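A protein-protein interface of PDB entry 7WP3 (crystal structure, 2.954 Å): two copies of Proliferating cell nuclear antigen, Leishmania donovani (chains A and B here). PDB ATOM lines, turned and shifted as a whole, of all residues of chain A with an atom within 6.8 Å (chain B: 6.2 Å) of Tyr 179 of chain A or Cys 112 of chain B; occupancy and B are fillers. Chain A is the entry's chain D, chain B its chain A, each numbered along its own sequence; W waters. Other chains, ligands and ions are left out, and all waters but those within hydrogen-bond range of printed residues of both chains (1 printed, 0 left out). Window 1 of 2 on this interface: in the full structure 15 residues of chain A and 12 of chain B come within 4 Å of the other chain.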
ATOM      1  N   GLU A 143       7.381 -38.381 -18.176  1.00  0.00           N
ATOM      2  CA  GLU A 143       7.571 -36.912 -18.295  1.00  0.00           C
ATOM      3  C   GLU A 143       9.076 -36.656 -18.228  1.00  0.00           C
ATOM      4  O   GLU A 143       9.594 -35.900 -19.076  1.00  0.00           O
ATOM      5  CB  GLU A 143       6.793 -36.130 -17.236  1.00  0.00           C
ATOM      6  CG  GLU A 143       6.925 -34.616 -17.376  1.00  0.00           C
ATOM      7  CD  GLU A 143       6.247 -34.000 -18.590  1.00  0.00           C
ATOM      8  OE1 GLU A 143       5.244 -34.571 -19.051  1.00  0.00           O
ATOM      9  OE2 GLU A 143       6.722 -32.947 -19.068  1.00  0.00           O
ATOM     10  N   ASP A 150      13.507 -33.846 -25.221  1.00  0.00           N
ATOM     11  CA  ASP A 150      13.193 -32.442 -25.604  1.00  0.00           C
ATOM     12  C   ASP A 150      14.428 -31.560 -25.422  1.00  0.00           C
ATOM     13  O   ASP A 150      14.855 -30.958 -26.417  1.00  0.00           O
ATOM     14  CB  ASP A 150      12.043 -31.853 -24.782  1.00  0.00           C
ATOM     15  CG  ASP A 150      10.697 -32.536 -24.984  1.00  0.00           C
ATOM     16  OD1 ASP A 150      10.678 -33.611 -25.654  1.00  0.00           O
ATOM     17  OD2 ASP A 150       9.672 -31.981 -24.476  1.00  0.00           O
ATOM     18  N   MET A 151      14.975 -31.471 -24.203  1.00  0.00           N
ATOM     19  CA  MET A 151      16.120 -30.559 -23.908  1.00  0.00           C
ATOM     20  C   MET A 151      17.258 -30.867 -24.887  1.00  0.00           C
ATOM     21  O   MET A 151      17.931 -29.924 -25.303  1.00  0.00           O
ATOM     22  CB  MET A 151      16.645 -30.679 -22.472  1.00  0.00           C
ATOM     23  CG  MET A 151      15.627 -30.332 -21.399  1.00  0.00           C
ATOM     24  SD  MET A 151      14.527 -28.932 -21.782  1.00  0.00           S
ATOM     25  CE  MET A 151      15.688 -27.584 -21.946  1.00  0.00           C
ATOM     26  N   PHE A 154      18.128 -29.097 -28.154  1.00  0.00           N
ATOM     27  CA  PHE A 154      18.840 -27.801 -27.965  1.00  0.00           C
ATOM     28  C   PHE A 154      20.345 -28.020 -27.766  1.00  0.00           C
ATOM     29  O   PHE A 154      21.129 -27.428 -28.528  1.00  0.00           O
ATOM     30  CB  PHE A 154      18.212 -27.001 -26.820  1.00  0.00           C
ATOM     31  CG  PHE A 154      16.783 -26.635 -27.102  1.00  0.00           C
ATOM     32  CD1 PHE A 154      16.494 -25.613 -27.991  1.00  0.00           C
ATOM     33  CD2 PHE A 154      15.739 -27.358 -26.549  1.00  0.00           C
ATOM     34  CE1 PHE A 154      15.182 -25.293 -28.295  1.00  0.00           C
ATOM     35  CE2 PHE A 154      14.426 -27.038 -26.852  1.00  0.00           C
ATOM     36  CZ  PHE A 154      14.150 -26.004 -27.722  1.00  0.00           C
ATOM     37  N   LYS A 168      12.967 -26.604 -12.803  1.00  0.00           N
ATOM     38  CA  LYS A 168      13.073 -26.007 -14.160  1.00  0.00           C
ATOM     39  C   LYS A 168      14.226 -26.695 -14.891  1.00  0.00           C
ATOM     40  O   LYS A 168      15.388 -26.430 -14.545  1.00  0.00           O
ATOM     41  CB  LYS A 168      13.321 -24.497 -14.092  1.00  0.00           C
ATOM     42  CG  LYS A 168      13.335 -23.770 -15.432  1.00  0.00           C
ATOM     43  CD  LYS A 168      14.219 -22.522 -15.449  1.00  0.00           C
ATOM     44  CE  LYS A 168      13.874 -21.507 -16.528  1.00  0.00           C
ATOM     45  NZ  LYS A 168      12.628 -20.759 -16.225  1.00  0.00           N
ATOM     46  N   PHE A 169      13.919 -27.510 -15.895  1.00  0.00           N
ATOM     47  CA  PHE A 169      14.931 -28.105 -16.796  1.00  0.00           C
ATOM     48  C   PHE A 169      15.177 -27.117 -17.940  1.00  0.00           C
ATOM     49  O   PHE A 169      14.210 -26.645 -18.537  1.00  0.00           O
ATOM     50  CB  PHE A 169      14.455 -29.466 -17.290  1.00  0.00           C
ATOM     51  CG  PHE A 169      14.039 -30.412 -16.202  1.00  0.00           C
ATOM     52  CD1 PHE A 169      12.744 -30.391 -15.709  1.00  0.00           C
ATOM     53  CD2 PHE A 169      14.921 -31.357 -15.706  1.00  0.00           C
ATOM     54  CE1 PHE A 169      12.340 -31.278 -14.725  1.00  0.00           C
ATOM     55  CE2 PHE A 169      14.516 -32.250 -14.725  1.00  0.00           C
ATOM     56  CZ  PHE A 169      13.228 -32.207 -14.234  1.00  0.00           C
ATOM     57  N   SER A 170      16.437 -26.800 -18.224  1.00  0.00           N
ATOM     58  CA  SER A 170      16.821 -25.783 -19.239  1.00  0.00           C
ATOM     59  C   SER A 170      18.022 -26.270 -20.057  1.00  0.00           C
ATOM     60  O   SER A 170      18.832 -27.043 -19.530  1.00  0.00           O
ATOM     61  CB  SER A 170      17.087 -24.465 -18.581  1.00  0.00           C
ATOM     62  OG  SER A 170      17.908 -24.652 -17.447  1.00  0.00           O
ATOM     63  N   SER A 171      18.110 -25.856 -21.322  1.00  0.00           N
ATOM     64  CA  SER A 171      19.214 -26.228 -22.253  1.00  0.00           C
ATOM     65  C   SER A 171      19.327 -25.190 -23.365  1.00  0.00           C
ATOM     66  O   SER A 171      18.337 -24.485 -23.582  1.00  0.00           O
ATOM     67  CB  SER A 171      19.019 -27.595 -22.834  1.00  0.00           C
ATOM     68  OG  SER A 171      20.072 -27.884 -23.741  1.00  0.00           O
ATOM     69  N   GLN A 177      17.322 -21.743 -27.450  1.00  0.00           N
ATOM     70  CA  GLN A 177      17.253 -22.008 -25.994  1.00  0.00           C
ATOM     71  C   GLN A 177      15.812 -22.370 -25.675  1.00  0.00           C
ATOM     72  O   GLN A 177      14.908 -21.797 -26.283  1.00  0.00           O
ATOM     73  CB  GLN A 177      17.759 -20.808 -25.195  1.00  0.00           C
ATOM     74  CG  GLN A 177      17.253 -19.480 -25.723  1.00  0.00           C
ATOM     75  CD  GLN A 177      17.992 -18.323 -25.104  1.00  0.00           C
ATOM     76  OE1 GLN A 177      18.865 -18.508 -24.261  1.00  0.00           O
ATOM     77  NE2 GLN A 177      17.630 -17.118 -25.518  1.00  0.00           N
ATOM     78  N   GLY A 178      15.634 -23.323 -24.773  1.00  0.00           N
ATOM     79  CA  GLY A 178      14.317 -23.735 -24.271  1.00  0.00           C
ATOM     80  C   GLY A 178      14.381 -24.118 -22.809  1.00  0.00           C
ATOM     81  O   GLY A 178      15.499 -24.264 -22.268  1.00  0.00           O
ATOM     82  N   TYR A 179      13.219 -24.288 -22.192  1.00  0.00           N
ATOM     83  CA  TYR A 179      13.101 -24.814 -20.815  1.00  0.00           C
ATOM     84  C   TYR A 179      11.730 -25.437 -20.605  1.00  0.00           C
ATOM     85  O   TYR A 179      10.776 -25.077 -21.294  1.00  0.00           O
ATOM     86  CB  TYR A 179      13.375 -23.711 -19.794  1.00  0.00           C
ATOM     87  CG  TYR A 179      12.248 -22.754 -19.506  1.00  0.00           C
ATOM     88  CD1 TYR A 179      11.182 -23.126 -18.707  1.00  0.00           C
ATOM     89  CD2 TYR A 179      12.294 -21.449 -19.971  1.00  0.00           C
ATOM     90  CE1 TYR A 179      10.161 -22.236 -18.420  1.00  0.00           C
ATOM     91  CE2 TYR A 179      11.297 -20.537 -19.669  1.00  0.00           C
ATOM     92  CZ  TYR A 179      10.220 -20.935 -18.895  1.00  0.00           C
ATOM     93  OH  TYR A 179       9.226 -20.037 -18.604  1.00  0.00           O
ATOM     94  N   THR A 180      11.653 -26.323 -19.623  1.00  0.00           N
ATOM     95  CA  THR A 180      10.382 -26.922 -19.171  1.00  0.00           C
ATOM     96  C   THR A 180      10.290 -26.681 -17.670  1.00  0.00           C
ATOM     97  O   THR A 180      11.139 -27.217 -16.966  1.00  0.00           O
ATOM     98  CB  THR A 180      10.320 -28.409 -19.532  1.00  0.00           C
ATOM     99  OG1 THR A 180      10.398 -28.487 -20.954  1.00  0.00           O
ATOM    100  CG2 THR A 180       9.056 -29.084 -19.048  1.00  0.00           C
ATOM    101  N   PHE A 181       9.314 -25.903 -17.205  1.00  0.00           N
ATOM    102  CA  PHE A 181       9.057 -25.732 -15.751  1.00  0.00           C
ATOM    103  C   PHE A 181       7.919 -26.657 -15.316  1.00  0.00           C
ATOM    104  O   PHE A 181       6.837 -26.608 -15.922  1.00  0.00           O
ATOM    105  CB  PHE A 181       8.717 -24.288 -15.389  1.00  0.00           C
ATOM    106  CG  PHE A 181       8.461 -24.102 -13.917  1.00  0.00           C
ATOM    107  CD1 PHE A 181       7.179 -24.191 -13.405  1.00  0.00           C
ATOM    108  CD2 PHE A 181       9.512 -23.898 -13.040  1.00  0.00           C
ATOM    109  CE1 PHE A 181       6.945 -24.037 -12.050  1.00  0.00           C
ATOM    110  CE2 PHE A 181       9.278 -23.753 -11.682  1.00  0.00           C
ATOM    111  CZ  PHE A 181       7.994 -23.826 -11.189  1.00  0.00           C
ATOM    112  N   ILE B  81       8.805 -31.313 -30.484  1.00  0.00           N
ATOM    113  CA  ILE B  81       8.853 -31.673 -29.028  1.00  0.00           C
ATOM    114  C   ILE B  81       7.839 -30.858 -28.239  1.00  0.00           C
ATOM    115  O   ILE B  81       8.065 -30.731 -27.040  1.00  0.00           O
ATOM    116  CB  ILE B  81      10.258 -31.570 -28.388  1.00  0.00           C
ATOM    117  CG1 ILE B  81      10.941 -30.205 -28.544  1.00  0.00           C
ATOM    118  CG2 ILE B  81      11.127 -32.705 -28.907  1.00  0.00           C
ATOM    119  CD1 ILE B  81      10.417 -29.116 -27.634  1.00  0.00           C
ATOM    120  N   VAL B  82       6.771 -30.372 -28.877  1.00  0.00           N
ATOM    121  CA  VAL B  82       5.629 -29.670 -28.211  1.00  0.00           C
ATOM    122  C   VAL B  82       4.400 -30.565 -28.343  1.00  0.00           C
ATOM    123  O   VAL B  82       4.045 -30.909 -29.476  1.00  0.00           O
ATOM    124  CB  VAL B  82       5.365 -28.271 -28.802  1.00  0.00           C
ATOM    125  CG1 VAL B  82       4.080 -27.669 -28.284  1.00  0.00           C
ATOM    126  CG2 VAL B  82       6.507 -27.312 -28.529  1.00  0.00           C
ATOM    127  N   ASP B  86      -1.237 -29.242 -25.760  1.00  0.00           N
ATOM    128  CA  ASP B  86      -0.711 -28.009 -25.123  1.00  0.00           C
ATOM    129  C   ASP B  86      -1.075 -26.816 -26.025  1.00  0.00           C
ATOM    130  O   ASP B  86      -1.264 -27.005 -27.232  1.00  0.00           O
ATOM    131  CB  ASP B  86       0.788 -28.126 -24.814  1.00  0.00           C
ATOM    132  CG  ASP B  86       1.128 -29.151 -23.737  1.00  0.00           C
ATOM    133  OD1 ASP B  86       0.206 -29.884 -23.298  1.00  0.00           O
ATOM    134  OD2 ASP B  86       2.317 -29.223 -23.349  1.00  0.00           O
ATOM    135  N   LEU B 101       8.153 -18.980 -28.092  1.00  0.00           N
ATOM    136  CA  LEU B 101       7.018 -19.919 -28.153  1.00  0.00           C
ATOM    137  C   LEU B 101       6.812 -20.402 -26.731  1.00  0.00           C
ATOM    138  O   LEU B 101       7.799 -20.880 -26.151  1.00  0.00           O
ATOM    139  CB  LEU B 101       7.354 -21.076 -29.095  1.00  0.00           C
ATOM    140  CG  LEU B 101       7.233 -20.758 -30.582  1.00  0.00           C
ATOM    141  CD1 LEU B 101       8.255 -19.723 -31.016  1.00  0.00           C
ATOM    142  CD2 LEU B 101       7.406 -22.020 -31.396  1.00  0.00           C
ATOM    143  N   THR B 102       5.606 -20.218 -26.192  1.00  0.00           N
ATOM    144  CA  THR B 102       5.291 -20.587 -24.790  1.00  0.00           C
ATOM    145  C   THR B 102       4.173 -21.631 -24.781  1.00  0.00           C
ATOM    146  O   THR B 102       3.122 -21.425 -25.429  1.00  0.00           O
ATOM    147  CB  THR B 102       5.026 -19.350 -23.930  1.00  0.00           C
ATOM    148  OG1 THR B 102       6.041 -18.388 -24.234  1.00  0.00           O
ATOM    149  CG2 THR B 102       5.037 -19.700 -22.457  1.00  0.00           C
ATOM    150  N   SER B 103       4.442 -22.737 -24.095  1.00  0.00           N
ATOM    151  CA  SER B 103       3.606 -23.958 -24.102  1.00  0.00           C
ATOM    152  C   SER B 103       3.057 -24.189 -22.700  1.00  0.00           C
ATOM    153  O   SER B 103       3.873 -24.400 -21.783  1.00  0.00           O
ATOM    154  CB  SER B 103       4.401 -25.143 -24.555  1.00  0.00           C
ATOM    155  OG  SER B 103       3.712 -26.343 -24.241  1.00  0.00           O
ATOM    156  N   GLU B 104       1.734 -24.169 -22.554  1.00  0.00           N
ATOM    157  CA  GLU B 104       1.044 -24.455 -21.271  1.00  0.00           C
ATOM    158  C   GLU B 104       0.250 -25.752 -21.421  1.00  0.00           C
ATOM    159  O   GLU B 104      -0.418 -25.939 -22.450  1.00  0.00           O
ATOM    160  CB  GLU B 104       0.112 -23.311 -20.861  1.00  0.00           C
ATOM    161  CG  GLU B 104       0.824 -22.083 -20.322  1.00  0.00           C
ATOM    162  CD  GLU B 104       1.235 -22.171 -18.866  1.00  0.00           C
ATOM    163  OE1 GLU B 104       1.229 -23.306 -18.315  1.00  0.00           O
ATOM    164  OE2 GLU B 104       1.567 -21.103 -18.295  1.00  0.00           O
ATOM    165  N   ARG B 110       2.395 -27.691 -16.292  1.00  0.00           N
ATOM    166  CA  ARG B 110       3.684 -27.633 -17.043  1.00  0.00           C
ATOM    167  C   ARG B 110       3.732 -26.383 -17.929  1.00  0.00           C
ATOM    168  O   ARG B 110       2.730 -26.060 -18.584  1.00  0.00           O
ATOM    169  CB  ARG B 110       3.867 -28.907 -17.871  1.00  0.00           C
ATOM    170  CG  ARG B 110       5.062 -28.888 -18.816  1.00  0.00           C
ATOM    171  CD  ARG B 110       5.151 -30.152 -19.657  1.00  0.00           C
ATOM    172  NE  ARG B 110       3.888 -30.426 -20.329  1.00  0.00           N
ATOM    173  CZ  ARG B 110       3.624 -31.486 -21.082  1.00  0.00           C
ATOM    174  NH1 ARG B 110       4.548 -32.407 -21.297  1.00  0.00           N
ATOM    175  NH2 ARG B 110       2.428 -31.606 -21.633  1.00  0.00           N
ATOM    176  N   LYS B 111       4.876 -25.710 -17.945  1.00  0.00           N
ATOM    177  CA  LYS B 111       5.128 -24.530 -18.806  1.00  0.00           C
ATOM    178  C   LYS B 111       6.446 -24.778 -19.539  1.00  0.00           C
ATOM    179  O   LYS B 111       7.487 -24.933 -18.864  1.00  0.00           O
ATOM    180  CB  LYS B 111       5.165 -23.235 -17.986  1.00  0.00           C
ATOM    181  CG  LYS B 111       5.144 -21.942 -18.801  1.00  0.00           C
ATOM    182  CD  LYS B 111       4.903 -20.663 -17.998  1.00  0.00           C
ATOM    183  CE  LYS B 111       6.171 -19.882 -17.698  1.00  0.00           C
ATOM    184  NZ  LYS B 111       6.643 -19.096 -18.867  1.00  0.00           N
ATOM    185  N   CYS B 112       6.400 -24.875 -20.866  1.00  0.00           N
ATOM    186  CA  CYS B 112       7.626 -24.901 -21.697  1.00  0.00           C
ATOM    187  C   CYS B 112       7.756 -23.554 -22.387  1.00  0.00           C
ATOM    188  O   CYS B 112       6.722 -23.045 -22.823  1.00  0.00           O
ATOM    189  CB  CYS B 112       7.572 -26.009 -22.730  1.00  0.00           C
ATOM    190  SG  CYS B 112       7.203 -27.607 -21.979  1.00  0.00           S
ATOM    191  N   GLU B 113       8.965 -23.010 -22.480  1.00  0.00           N
ATOM    192  CA  GLU B 113       9.201 -21.780 -23.268  1.00  0.00           C
ATOM    193  C   GLU B 113      10.501 -21.928 -24.056  1.00  0.00           C
ATOM    194  O   GLU B 113      11.538 -22.222 -23.456  1.00  0.00           O
ATOM    195  CB  GLU B 113       9.208 -20.551 -22.363  1.00  0.00           C
ATOM    196  CG  GLU B 113       9.606 -19.265 -23.073  1.00  0.00           C
ATOM    197  CD  GLU B 113       9.798 -18.057 -22.167  1.00  0.00           C
ATOM    198  OE1 GLU B 113       8.850 -17.735 -21.401  1.00  0.00           O
ATOM    199  OE2 GLU B 113      10.905 -17.445 -22.223  1.00  0.00           O
ATOM    200  N   TYR B 114      10.440 -21.661 -25.357  1.00  0.00           N
ATOM    201  CA  TYR B 114      11.591 -21.755 -26.284  1.00  0.00           C
ATOM    202  C   TYR B 114      11.801 -20.396 -26.962  1.00  0.00           C
ATOM    203  O   TYR B 114      10.826 -19.696 -27.234  1.00  0.00           O
ATOM    204  CB  TYR B 114      11.323 -22.887 -27.275  1.00  0.00           C
ATOM    205  CG  TYR B 114      10.756 -24.140 -26.660  1.00  0.00           C
ATOM    206  CD1 TYR B 114      11.568 -25.040 -25.992  1.00  0.00           C
ATOM    207  CD2 TYR B 114       9.415 -24.444 -26.764  1.00  0.00           C
ATOM    208  CE1 TYR B 114      11.070 -26.208 -25.435  1.00  0.00           C
ATOM    209  CE2 TYR B 114       8.900 -25.611 -26.222  1.00  0.00           C
ATOM    210  CZ  TYR B 114       9.724 -26.499 -25.555  1.00  0.00           C
ATOM    211  OH  TYR B 114       9.209 -27.640 -25.006  1.00  0.00           O
HETATM  212  O   HOH W   1      11.096 -28.965 -23.784  1.00  0.00           O
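Among the printed residues, pairs that only touch across the chains: Phe 154 of chain A with Tyr 114 of chain B, Gln 177 of chain A with Tyr 114 of chain B, Gly 178 of chain A with Glu 113 of chain B, Gly 178 of chain A with Tyr 114 of chain B, Tyr 179 of chain A with Cys 112 of chain B, Thr 180 of chain A with Lys 111 of chain B and Phe 181 of chain A with Arg 110 of chain B.
Of the printed residues of chain B, Glu 143 of chain A touches Arg 110 (3.2 Å). Of the printed residues of chain B, Gln 177 of chain A touches Tyr 114 (3.3 Å). Printed residues of chain B within 4 Å of Gly 178 of chain A: Glu 113 and Tyr 114. Tyr 179 of chain A touches just these residues of chain B: Lys 111, Cys 112 and Glu 113. Of the printed residues of chain A, Ile 81 of chain B touches Asp 150 (3.3 Å). Asp 86 of chain B touches none of the printed residues of chain A. Glu 104 of chain B touches none of the printed residues of chain A. Of the printed residues of chain A, Lys 111 of chain B touches Tyr 179, Thr 180 and Phe 181. Cys 112 of chain B touches just these residues of chain A: Tyr 179 and Thr 180. The nearest printed residue of chain A that does not touch Tyr 114 of chain B is Tyr 179 of chain A (4.2 Å).
The side-chain carboxylate (OE2) of Glu 143 of chain A is in salt-bridge range of the guanidinium group (NH1) of Arg 110 of chain B. O of Glu 113 of chain B sits at hydrogen-bond distance from N of Tyr 179 of chain A (2.9 Å). The side-chain sulfur (SG) of Cys 112 of chain B lies within hydrogen-bond range of the side-chain hydroxyl (OG1) of Thr 180 of chain A. The side-chain amino group (NZ) of Lys 111 of chain B is in hydrogen-bond range of the side-chain hydroxyl (OH) of Tyr 179 of chain A (2.8 Å). The backbone NH (N) of Phe 181 of chain A sits at hydrogen-bond distance from the backbone carbonyl oxygen (O) of Lys 111 of chain B (2.7 Å). The side-chain carboxylate (OD2) of Asp 150 of chain A sits close to the backbone carbonyl oxygen (O) of Ile 81 of chain B.
The backbone carbonyl oxygen (O) of Ser 171 of chain A lies within hydrogen-bond range of the backbone NH (N) of Gly 178 of chain A (3.2 Å). The backbone NH of Thr 180 of chain A lies within hydrogen-bond range of the backbone carbonyl oxygen of Phe 169 of chain A (2.8 Å). The side-chain sulfur of Cys 112 of chain B lies close to the side-chain hydroxyl of Tyr 114 of chain B. The backbone NH of Ser 103 of chain B is in hydrogen-bond range of the backbone carbonyl oxygen of Cys 112 of chain B, 2.6 Å away. The backbone carbonyl oxygen (O) of Leu 101 of chain B sits at hydrogen-bond distance from the backbone NH (N) of Tyr 114 of chain B (2.9 Å). The side-chain carboxylate (OD2) of Asp 86 of chain B is in salt-bridge range of the guanidinium group (NH2) of Arg 110 of chain B (2.9 Å).
No position is printed for both chains. Of the 13 pairs that touch across the chains among the printed residues, none has its exchanged pair printed and touching as well.
Of the 13 printed residues of chain A, 8 touch a printed residue of chain B. Printed residues of chain A that touch a printed residue of chain B: Glu 143, Asp 150, Phe 154, Gln 177, Gly 178, Tyr 179, Thr 180 and Phe 181. Hydrophobic or aromatic side chains of chain A within 4 Å of the printed part of chain B: Phe 154, Tyr 179 and Phe 181. Printed residues of chain B that touch a printed residue of chain A: Ile 81, Arg 110, Lys 111, Cys 112, Glu 113 and Tyr 114. Hydrophobic or aromatic side chains of chain B within 4 Å of the printed part of chain A: Ile 81 and Tyr 114.
Water W1 lies within hydrogen-bond range of OH of Tyr 114 of chain B (2.6 Å), OG1 of Thr 180 of chain A (3.0 Å) and OD2 of Asp 150 of chain A (3.4 Å).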
